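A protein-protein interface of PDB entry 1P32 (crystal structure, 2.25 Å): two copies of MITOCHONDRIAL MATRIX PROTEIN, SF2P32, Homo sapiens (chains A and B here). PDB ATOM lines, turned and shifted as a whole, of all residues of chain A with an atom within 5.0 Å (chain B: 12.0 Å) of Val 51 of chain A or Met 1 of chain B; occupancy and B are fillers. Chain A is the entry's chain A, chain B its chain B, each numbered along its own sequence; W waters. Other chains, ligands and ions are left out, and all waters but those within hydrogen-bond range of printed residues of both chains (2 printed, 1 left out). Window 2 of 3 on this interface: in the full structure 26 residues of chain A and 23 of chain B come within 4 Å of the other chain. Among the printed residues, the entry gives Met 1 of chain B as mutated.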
ATOM      1  N   ARG A  49      35.775   6.974 -25.776  1.00  0.00           N
ATOM      2  CA  ARG A  49      36.404   5.873 -25.071  1.00  0.00           C
ATOM      3  C   ARG A  49      35.338   4.940 -24.510  1.00  0.00           C
ATOM      4  O   ARG A  49      34.263   5.387 -24.111  1.00  0.00           O
ATOM      5  CB  ARG A  49      37.259   6.450 -23.945  1.00  0.00           C
ATOM      6  CG  ARG A  49      37.930   5.447 -23.060  1.00  0.00           C
ATOM      7  CD  ARG A  49      38.961   6.149 -22.206  1.00  0.00           C
ATOM      8  NE  ARG A  49      39.750   5.197 -21.439  1.00  0.00           N
ATOM      9  CZ  ARG A  49      39.340   4.606 -20.325  1.00  0.00           C
ATOM     10  NH1 ARG A  49      38.138   4.868 -19.834  1.00  0.00           N
ATOM     11  NH2 ARG A  49      40.136   3.742 -19.708  1.00  0.00           N
ATOM     12  N   LYS A  50      35.635   3.642 -24.499  1.00  0.00           N
ATOM     13  CA  LYS A  50      34.708   2.655 -23.968  1.00  0.00           C
ATOM     14  C   LYS A  50      35.335   1.800 -22.872  1.00  0.00           C
ATOM     15  O   LYS A  50      36.525   1.511 -22.896  1.00  0.00           O
ATOM     16  CB  LYS A  50      34.181   1.748 -25.086  1.00  0.00           C
ATOM     17  CG  LYS A  50      33.268   2.465 -26.076  1.00  0.00           C
ATOM     18  CD  LYS A  50      32.631   1.502 -27.065  1.00  0.00           C
ATOM     19  CE  LYS A  50      31.649   2.237 -27.967  1.00  0.00           C
ATOM     20  NZ  LYS A  50      30.991   1.343 -28.963  1.00  0.00           N
ATOM     21  N   VAL A  51      34.519   1.417 -21.899  1.00  0.00           N
ATOM     22  CA  VAL A  51      34.955   0.569 -20.797  1.00  0.00           C
ATOM     23  C   VAL A  51      33.798  -0.378 -20.547  1.00  0.00           C
ATOM     24  O   VAL A  51      32.722  -0.212 -21.131  1.00  0.00           O
ATOM     25  CB  VAL A  51      35.232   1.371 -19.504  1.00  0.00           C
ATOM     26  CG1 VAL A  51      36.336   2.384 -19.748  1.00  0.00           C
ATOM     27  CG2 VAL A  51      33.958   2.065 -19.037  1.00  0.00           C
ATOM     28  N   ALA A  52      34.012  -1.362 -19.681  1.00  0.00           N
ATOM     29  CA  ALA A  52      32.977  -2.335 -19.380  1.00  0.00           C
ATOM     30  C   ALA A  52      31.629  -1.653 -19.156  1.00  0.00           C
ATOM     31  O   ALA A  52      31.482  -0.835 -18.253  1.00  0.00           O
ATOM     32  CB  ALA A  52      33.372  -3.158 -18.148  1.00  0.00           C
ATOM     33  N   GLY A  53      30.668  -1.977 -20.017  1.00  0.00           N
ATOM     34  CA  GLY A  53      29.320  -1.433 -19.914  1.00  0.00           C
ATOM     35  C   GLY A  53      29.096   0.052 -20.144  1.00  0.00           C
ATOM     36  O   GLY A  53      27.983   0.546 -19.934  1.00  0.00           O
ATOM     37  N   GLU A  54      30.118   0.769 -20.599  1.00  0.00           N
ATOM     38  CA  GLU A  54      29.963   2.205 -20.803  1.00  0.00           C
ATOM     39  C   GLU A  54      30.685   2.816 -21.994  1.00  0.00           C
ATOM     40  O   GLU A  54      31.706   2.312 -22.456  1.00  0.00           O
ATOM     41  CB  GLU A  54      30.438   2.946 -19.553  1.00  0.00           C
ATOM     42  CG  GLU A  54      29.628   2.698 -18.302  1.00  0.00           C
ATOM     43  CD  GLU A  54      30.308   3.270 -17.069  1.00  0.00           C
ATOM     44  OE1 GLU A  54      30.840   4.395 -17.160  1.00  0.00           O
ATOM     45  OE2 GLU A  54      30.303   2.607 -16.013  1.00  0.00           O
ATOM     46  N   ILE A  56      32.188   6.594 -23.059  1.00  0.00           N
ATOM     47  CA  ILE A  56      32.517   7.912 -22.526  1.00  0.00           C
ATOM     48  C   ILE A  56      32.873   8.840 -23.677  1.00  0.00           C
ATOM     49  O   ILE A  56      33.738   8.521 -24.486  1.00  0.00           O
ATOM     50  CB  ILE A  56      33.741   7.859 -21.575  1.00  0.00           C
ATOM     51  CG1 ILE A  56      33.554   6.772 -20.503  1.00  0.00           C
ATOM     52  CG2 ILE A  56      33.936   9.223 -20.920  1.00  0.00           C
ATOM     53  CD1 ILE A  56      32.355   6.978 -19.613  1.00  0.00           C
ATOM     54  N   LYS A 101      25.530   4.530 -19.929  1.00  0.00           N
ATOM     55  CA  LYS A 101      25.494   3.176 -19.393  1.00  0.00           C
ATOM     56  C   LYS A 101      24.814   2.356 -20.484  1.00  0.00           C
ATOM     57  O   LYS A 101      23.656   2.606 -20.816  1.00  0.00           O
ATOM     58  CB  LYS A 101      24.636   3.105 -18.124  1.00  0.00           C
ATOM     59  CG  LYS A 101      25.187   3.813 -16.898  1.00  0.00           C
ATOM     60  CD  LYS A 101      26.395   3.096 -16.352  1.00  0.00           C
ATOM     61  CE  LYS A 101      26.796   3.619 -14.981  1.00  0.00           C
ATOM     62  NZ  LYS A 101      27.919   2.812 -14.402  1.00  0.00           N
ATOM     63  N   ASP A 172      37.511   8.030 -12.523  1.00  0.00           N
ATOM     64  CA  ASP A 172      37.448   6.578 -12.721  1.00  0.00           C
ATOM     65  C   ASP A 172      37.182   6.215 -14.182  1.00  0.00           C
ATOM     66  O   ASP A 172      37.377   5.074 -14.593  1.00  0.00           O
ATOM     67  CB  ASP A 172      36.361   5.958 -11.830  1.00  0.00           C
ATOM     68  CG  ASP A 172      36.789   5.838 -10.362  1.00  0.00           C
ATOM     69  OD1 ASP A 172      35.940   5.476  -9.523  1.00  0.00           O
ATOM     70  OD2 ASP A 172      37.969   6.090 -10.044  1.00  0.00           O
ATOM     71  N   ARG A 173      36.725   7.192 -14.957  1.00  0.00           N
ATOM     72  CA  ARG A 173      36.451   6.988 -16.367  1.00  0.00           C
ATOM     73  C   ARG A 173      37.499   7.670 -17.240  1.00  0.00           C
ATOM     74  O   ARG A 173      37.307   7.839 -18.444  1.00  0.00           O
ATOM     75  CB  ARG A 173      35.045   7.488 -16.708  1.00  0.00           C
ATOM     76  CG  ARG A 173      33.961   6.406 -16.621  1.00  0.00           C
ATOM     77  CD  ARG A 173      32.775   6.844 -15.781  1.00  0.00           C
ATOM     78  NE  ARG A 173      33.053   6.689 -14.359  1.00  0.00           N
ATOM     79  CZ  ARG A 173      32.573   5.707 -13.602  1.00  0.00           C
ATOM     80  NH1 ARG A 173      31.779   4.780 -14.123  1.00  0.00           N
ATOM     81  NH2 ARG A 173      32.915   5.634 -12.328  1.00  0.00           N
ATOM     82  N   MET B   1      30.785  -0.059 -15.710  1.00  0.00           N
ATOM     83  CA  MET B   1      31.667  -0.266 -14.524  1.00  0.00           C
ATOM     84  C   MET B   1      30.943   0.046 -13.230  1.00  0.00           C
ATOM     85  O   MET B   1      29.902   0.697 -13.226  1.00  0.00           O
ATOM     86  CB  MET B   1      32.905   0.635 -14.560  1.00  0.00           C
ATOM     87  CG  MET B   1      33.910   0.386 -15.655  1.00  0.00           C
ATOM     88  SD  MET B   1      35.454   1.283 -15.280  1.00  0.00           S
ATOM     89  CE  MET B   1      34.847   2.994 -15.033  1.00  0.00           C
ATOM     90  N   HIS B   2      31.535  -0.410 -12.134  1.00  0.00           N
ATOM     91  CA  HIS B   2      31.002  -0.201 -10.796  1.00  0.00           C
ATOM     92  C   HIS B   2      32.224  -0.295  -9.879  1.00  0.00           C
ATOM     93  O   HIS B   2      32.412  -1.289  -9.185  1.00  0.00           O
ATOM     94  CB  HIS B   2      29.993  -1.305 -10.464  1.00  0.00           C
ATOM     95  CG  HIS B   2      29.018  -0.941  -9.383  1.00  0.00           C
ATOM     96  ND1 HIS B   2      28.010  -1.791  -8.979  1.00  0.00           N
ATOM     97  CD2 HIS B   2      28.876   0.186  -8.647  1.00  0.00           C
ATOM     98  CE1 HIS B   2      27.288  -1.202  -8.041  1.00  0.00           C
ATOM     99  NE2 HIS B   2      27.792  -0.001  -7.821  1.00  0.00           N
ATOM    100  N   THR B   3      33.059   0.743  -9.907  1.00  0.00           N
ATOM    101  CA  THR B   3      34.285   0.807  -9.107  1.00  0.00           C
ATOM    102  C   THR B   3      34.002   0.992  -7.618  1.00  0.00           C
ATOM    103  O   THR B   3      32.850   1.095  -7.203  1.00  0.00           O
ATOM    104  CB  THR B   3      35.177   1.979  -9.557  1.00  0.00           C
ATOM    105  OG1 THR B   3      34.523   3.216  -9.256  1.00  0.00           O
ATOM    106  CG2 THR B   3      35.427   1.914 -11.056  1.00  0.00           C
ATOM    107  N   ASP B   4      35.056   1.041  -6.812  1.00  0.00           N
ATOM    108  CA  ASP B   4      34.861   1.232  -5.381  1.00  0.00           C
ATOM    109  C   ASP B   4      34.392   2.662  -5.159  1.00  0.00           C
ATOM    110  O   ASP B   4      33.578   2.933  -4.276  1.00  0.00           O
ATOM    111  CB  ASP B   4      36.153   0.972  -4.597  1.00  0.00           C
ATOM    112  CG  ASP B   4      36.617  -0.469  -4.701  1.00  0.00           C
ATOM    113  OD1 ASP B   4      35.755  -1.376  -4.691  1.00  0.00           O
ATOM    114  OD2 ASP B   4      37.844  -0.697  -4.764  1.00  0.00           O
ATOM    115  N   GLY B   5      34.914   3.572  -5.974  1.00  0.00           N
ATOM    116  CA  GLY B   5      34.526   4.960  -5.878  1.00  0.00           C
ATOM    117  C   GLY B   5      33.038   5.073  -6.125  1.00  0.00           C
ATOM    118  O   GLY B   5      32.345   5.797  -5.415  1.00  0.00           O
ATOM    119  N   ASP B   6      32.533   4.341  -7.115  1.00  0.00           N
ATOM    120  CA  ASP B   6      31.103   4.399  -7.419  1.00  0.00           C
ATOM    121  C   ASP B   6      30.262   3.923  -6.238  1.00  0.00           C
ATOM    122  O   ASP B   6      29.215   4.505  -5.939  1.00  0.00           O
ATOM    123  CB  ASP B   6      30.754   3.553  -8.652  1.00  0.00           C
ATOM    124  CG  ASP B   6      31.488   4.001  -9.908  1.00  0.00           C
ATOM    125  OD1 ASP B   6      31.740   5.216 -10.076  1.00  0.00           O
ATOM    126  OD2 ASP B   6      31.781   3.131 -10.753  1.00  0.00           O
ATOM    127  N   LYS B   7      30.716   2.861  -5.576  1.00  0.00           N
ATOM    128  CA  LYS B   7      30.002   2.309  -4.424  1.00  0.00           C
ATOM    129  C   LYS B   7      29.981   3.285  -3.250  1.00  0.00           C
ATOM    130  O   LYS B   7      28.968   3.419  -2.564  1.00  0.00           O
ATOM    131  CB  LYS B   7      30.631   0.984  -3.986  1.00  0.00           C
ATOM    132  CG  LYS B   7      30.552  -0.112  -5.050  1.00  0.00           C
ATOM    133  CD  LYS B   7      31.089  -1.438  -4.525  1.00  0.00           C
ATOM    134  CE  LYS B   7      31.004  -2.546  -5.570  1.00  0.00           C
ATOM    135  NZ  LYS B   7      31.889  -2.296  -6.739  1.00  0.00           N
ATOM    136  N   ALA B   8      31.100   3.964  -3.014  1.00  0.00           N
ATOM    137  CA  ALA B   8      31.151   4.938  -1.928  1.00  0.00           C
ATOM    138  C   ALA B   8      30.206   6.086  -2.291  1.00  0.00           C
ATOM    139  O   ALA B   8      29.545   6.652  -1.429  1.00  0.00           O
ATOM    140  CB  ALA B   8      32.563   5.458  -1.756  1.00  0.00           C
ATOM    141  N   PHE B   9      30.143   6.395  -3.585  1.00  0.00           N
ATOM    142  CA  PHE B   9      29.301   7.463  -4.108  1.00  0.00           C
ATOM    143  C   PHE B   9      27.844   7.124  -3.789  1.00  0.00           C
ATOM    144  O   PHE B   9      27.091   7.973  -3.297  1.00  0.00           O
ATOM    145  CB  PHE B   9      29.503   7.574  -5.630  1.00  0.00           C
ATOM    146  CG  PHE B   9      29.001   8.866  -6.249  1.00  0.00           C
ATOM    147  CD1 PHE B   9      28.257   9.787  -5.515  1.00  0.00           C
ATOM    148  CD2 PHE B   9      29.259   9.142  -7.593  1.00  0.00           C
ATOM    149  CE1 PHE B   9      27.776  10.966  -6.109  1.00  0.00           C
ATOM    150  CE2 PHE B   9      28.787  10.311  -8.200  1.00  0.00           C
ATOM    151  CZ  PHE B   9      28.040  11.226  -7.454  1.00  0.00           C
ATOM    152  N   VAL B  10      27.459   5.877  -4.064  1.00  0.00           N
ATOM    153  CA  VAL B  10      26.092   5.417  -3.821  1.00  0.00           C
ATOM    154  C   VAL B  10      25.702   5.507  -2.350  1.00  0.00           C
ATOM    155  O   VAL B  10      24.615   5.978  -2.028  1.00  0.00           O
ATOM    156  CB  VAL B  10      25.888   3.953  -4.309  1.00  0.00           C
ATOM    157  CG1 VAL B  10      24.520   3.445  -3.873  1.00  0.00           C
ATOM    158  CG2 VAL B  10      25.998   3.891  -5.826  1.00  0.00           C
ATOM    159  N   LEU B 202      20.460   9.903  -9.981  1.00  0.00           N
ATOM    160  CA  LEU B 202      21.913   9.793 -10.009  1.00  0.00           C
ATOM    161  C   LEU B 202      22.354   8.518  -9.309  1.00  0.00           C
ATOM    162  O   LEU B 202      23.293   7.858  -9.746  1.00  0.00           O
ATOM    163  CB  LEU B 202      22.548  11.009  -9.320  1.00  0.00           C
ATOM    164  CG  LEU B 202      24.074  11.153  -9.311  1.00  0.00           C
ATOM    165  CD1 LEU B 202      24.618  11.244 -10.748  1.00  0.00           C
ATOM    166  CD2 LEU B 202      24.441  12.410  -8.529  1.00  0.00           C
ATOM    167  N   LYS B 203      21.667   8.178  -8.222  1.00  0.00           N
ATOM    168  CA  LYS B 203      21.989   6.980  -7.455  1.00  0.00           C
ATOM    169  C   LYS B 203      21.735   5.733  -8.291  1.00  0.00           C
ATOM    170  O   LYS B 203      22.569   4.828  -8.332  1.00  0.00           O
ATOM    171  CB  LYS B 203      21.148   6.919  -6.173  1.00  0.00           C
ATOM    172  CG  LYS B 203      21.384   5.663  -5.338  1.00  0.00           C
ATOM    173  CD  LYS B 203      20.459   5.615  -4.127  1.00  0.00           C
ATOM    174  CE  LYS B 203      20.586   4.296  -3.385  1.00  0.00           C
ATOM    175  NZ  LYS B 203      19.617   4.196  -2.253  1.00  0.00           N
ATOM    176  N   SER B 204      20.580   5.692  -8.952  1.00  0.00           N
ATOM    177  CA  SER B 204      20.217   4.561  -9.803  1.00  0.00           C
ATOM    178  C   SER B 204      21.196   4.413 -10.965  1.00  0.00           C
ATOM    179  O   SER B 204      21.540   3.302 -11.359  1.00  0.00           O
ATOM    180  CB  SER B 204      18.807   4.749 -10.366  1.00  0.00           C
ATOM    181  OG  SER B 204      17.851   4.850  -9.325  1.00  0.00           O
ATOM    182  N   PHE B 205      21.639   5.544 -11.504  1.00  0.00           N
ATOM    183  CA  PHE B 205      22.569   5.549 -12.627  1.00  0.00           C
ATOM    184  C   PHE B 205      23.922   4.980 -12.218  1.00  0.00           C
ATOM    185  O   PHE B 205      24.421   4.028 -12.817  1.00  0.00           O
ATOM    186  CB  PHE B 205      22.764   6.975 -13.127  1.00  0.00           C
ATOM    187  CG  PHE B 205      23.616   7.077 -14.360  1.00  0.00           C
ATOM    188  CD1 PHE B 205      23.087   6.767 -15.614  1.00  0.00           C
ATOM    189  CD2 PHE B 205      24.946   7.495 -14.271  1.00  0.00           C
ATOM    190  CE1 PHE B 205      23.869   6.877 -16.768  1.00  0.00           C
ATOM    191  CE2 PHE B 205      25.737   7.606 -15.416  1.00  0.00           C
ATOM    192  CZ  PHE B 205      25.193   7.296 -16.669  1.00  0.00           C
ATOM    193  N   VAL B 206      24.511   5.577 -11.188  1.00  0.00           N
ATOM    194  CA  VAL B 206      25.814   5.158 -10.687  1.00  0.00           C
ATOM    195  C   VAL B 206      25.784   3.718 -10.189  1.00  0.00           C
ATOM    196  O   VAL B 206      26.804   3.038 -10.157  1.00  0.00           O
ATOM    197  CB  VAL B 206      26.273   6.083  -9.538  1.00  0.00           C
ATOM    198  CG1 VAL B 206      27.616   5.613  -8.979  1.00  0.00           C
ATOM    199  CG2 VAL B 206      26.370   7.519 -10.048  1.00  0.00           C
ATOM    200  N   LYS B 207      24.595   3.260  -9.820  1.00  0.00           N
ATOM    201  CA  LYS B 207      24.414   1.918  -9.305  1.00  0.00           C
ATOM    202  C   LYS B 207      24.337   0.895 -10.445  1.00  0.00           C
ATOM    203  O   LYS B 207      24.768  -0.250 -10.284  1.00  0.00           O
ATOM    204  CB  LYS B 207      23.130   1.890  -8.466  1.00  0.00           C
ATOM    205  CG  LYS B 207      23.028   0.761  -7.474  1.00  0.00           C
ATOM    206  CD  LYS B 207      21.735   0.860  -6.672  1.00  0.00           C
ATOM    207  CE  LYS B 207      21.676  -0.218  -5.604  1.00  0.00           C
ATOM    208  NZ  LYS B 207      21.823  -1.578  -6.193  1.00  0.00           N
ATOM    209  N   SER B 208      23.814   1.322 -11.598  1.00  0.00           N
ATOM    210  CA  SER B 208      23.651   0.445 -12.756  1.00  0.00           C
ATOM    211  C   SER B 208      24.955   0.026 -13.437  1.00  0.00           C
ATOM    212  O   SER B 208      26.005   0.638 -13.221  1.00  0.00           O
ATOM    213  CB  SER B 208      22.729   1.104 -13.793  1.00  0.00           C
ATOM    214  OG  SER B 208      23.338   2.245 -14.377  1.00  0.00           O
ATOM    215  N   GLN B 209      24.847  -1.013 -14.273  1.00  0.00           N
ATOM    216  CA  GLN B 209      25.945  -1.616 -15.044  1.00  0.00           C
ATOM    217  C   GLN B 209      26.800  -2.598 -14.257  1.00  0.00           C
ATOM    218  O   GLN B 209      26.512  -2.817 -13.061  1.00  0.00           O
ATOM    219  CB  GLN B 209      26.854  -0.553 -15.650  1.00  0.00           C
ATOM    220  CG  GLN B 209      26.245   0.208 -16.783  1.00  0.00           C
ATOM    221  CD  GLN B 209      25.983  -0.648 -17.989  1.00  0.00           C
ATOM    222  OE1 GLN B 209      26.874  -1.330 -18.483  1.00  0.00           O
ATOM    223  NE2 GLN B 209      24.758  -0.605 -18.486  1.00  0.00           N
ATOM    224  OXT GLN B 209      27.754  -3.142 -14.856  1.00  0.00           O
HETATM  225  O   HOH W   1      37.630   4.380  -7.298  1.00  0.00           O
HETATM  226  O   HOH W   2      33.467   6.824  -8.852  1.00  0.00           O
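Hydrophobic or aromatic side chains of chain A that line the printed part of chain B: Val 51.
Of the 18 printed residues of chain B, 7 touch a printed residue of chain A.
Hydrophobic or aromatic side chains of chain B within 4 Å of the printed part of chain A: Met 1 and Phe 205.
Among the printed residues, 13 pairs touch across the chains.
The side-chain carboxylate (OE2) of Glu 54 of chain A lies within salt-bridge range of the side-chain amino group (NZ) of Lys 101 of chain A, 2.9 Å away.
The backbone NH (N) of Gly 5 of chain B sits close to the side-chain hydroxyl (OG1) of Thr 3 of chain B (3.3 Å).
The backbone carbonyl oxygen (O) of Phe 205 of chain B lies within hydrogen-bond range of the side-chain hydroxyl (OG) of Ser 208 of chain B (2.6 Å).
The backbone NH (N) of Thr 3 of chain B lies within hydrogen-bond range of the side-chain carboxylate (OD2) of Asp 6 of chain B (2.8 Å).
The backbone carbonyl oxygen (O) of Arg 173 of chain A sits at hydrogen-bond distance from the guanidinium group (NH1) of Arg 49 of chain A.
NH1 of Arg 173 of chain A is in salt-bridge range of OE1 of Glu 54 of chain A (3.2 Å).
Among the printed residues, pairs that only touch across the chains: Val 51 of chain A with Met 1 of chain B (3.8 Å), Lys 101 of chain A with Phe 205 of chain B (3.2 Å), Lys 101 of chain A with Gln 209 of chain B (2.9 Å), Asp 172 of chain A with Met 1 of chain B (3.3 Å), Asp 172 of chain A with Gly 5 of chain B (3.9 Å) and Arg 173 of chain A with Met 1 of chain B (3.7 Å).
No position is printed for both chains.
Of the 13 pairs that touch across the chains among the printed residues, none has its exchanged pair printed and touching as well.
OE2 of Glu 54 of chain A sits at hydrogen-bond distance from N of Met 1 of chain B (2.7 Å).
The side-chain carboxylate (OD1) of Asp 6 of chain B lies within salt-bridge range of the guanidinium group (NH2) of Arg 173 of chain A (2.6 Å).
The backbone carbonyl oxygen (O) of Gly 53 of chain A lies close to the side-chain amide oxygen (OE1) of Gln 209 of chain B, at 2.6 Å.
The side-chain amino group (NZ) of Lys 101 of chain A sits at hydrogen-bond distance from the backbone carbonyl oxygen (O) of Met 1 of chain B, at 3.1 Å.
The backbone NH (N) of Met 1 of chain B sits at hydrogen-bond distance from the backbone carbonyl oxygen (O) of Ala 52 of chain A (2.7 Å).
NZ of Lys 101 of chain A lies within hydrogen-bond range of O of Ser 208 of chain B.
The side-chain hydroxyl (OG1) of Thr 3 of chain B lies within hydrogen-bond range of the side-chain carboxylate (OD1) of Asp 172 of chain A, at 2.7 Å.
Water W2 lies within hydrogen-bond range of OD1 of Asp 6 of chain B (2.7 Å) and OD1 of Asp 172 of chain A (2.9 Å).
Water W1 bridges OD1 of Asp 172 of chain A (3.0 Å) and N of Gly 5 of chain B (3.1 Å).
Of chain B, only Met 1 (3.8 Å) comes within 4 Å of Val 51 of chain A.
Of the printed residues of chain A, Met 1 of chain B touches Val 51, Ala 52, Glu 54, Lys 101, Asp 172 and Arg 173.
No residue of chain B comes within 4 Å of Arg 49 of chain A.
No residue of chain B comes within 4 Å of Lys 50 of chain A.
Ala 52 of chain A touches one residue of chain B.
Gly 53 of chain A touches one residue of chain B.
Arg 173 of chain A touches just these residues of chain B: Met 1 and Asp 6.
Of the printed residues of chain A, Gly 5 of chain B touches Asp 172.
Of the printed residues of chain B, Lys 101 of chain A touches Met 1, Phe 205, Ser 208 and Gln 209.
Printed residues of chain A within 4 Å of Asp 6 of chain B: Arg 173 (2.6 Å).
Asp 4 of chain B touches none of the printed residues of chain A.
Val 10 of chain B touches none of the printed residues of chain A.
The nearest residue of chain B that does not touch Val 51 of chain A is Gln 209 of chain B (6.5 Å).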
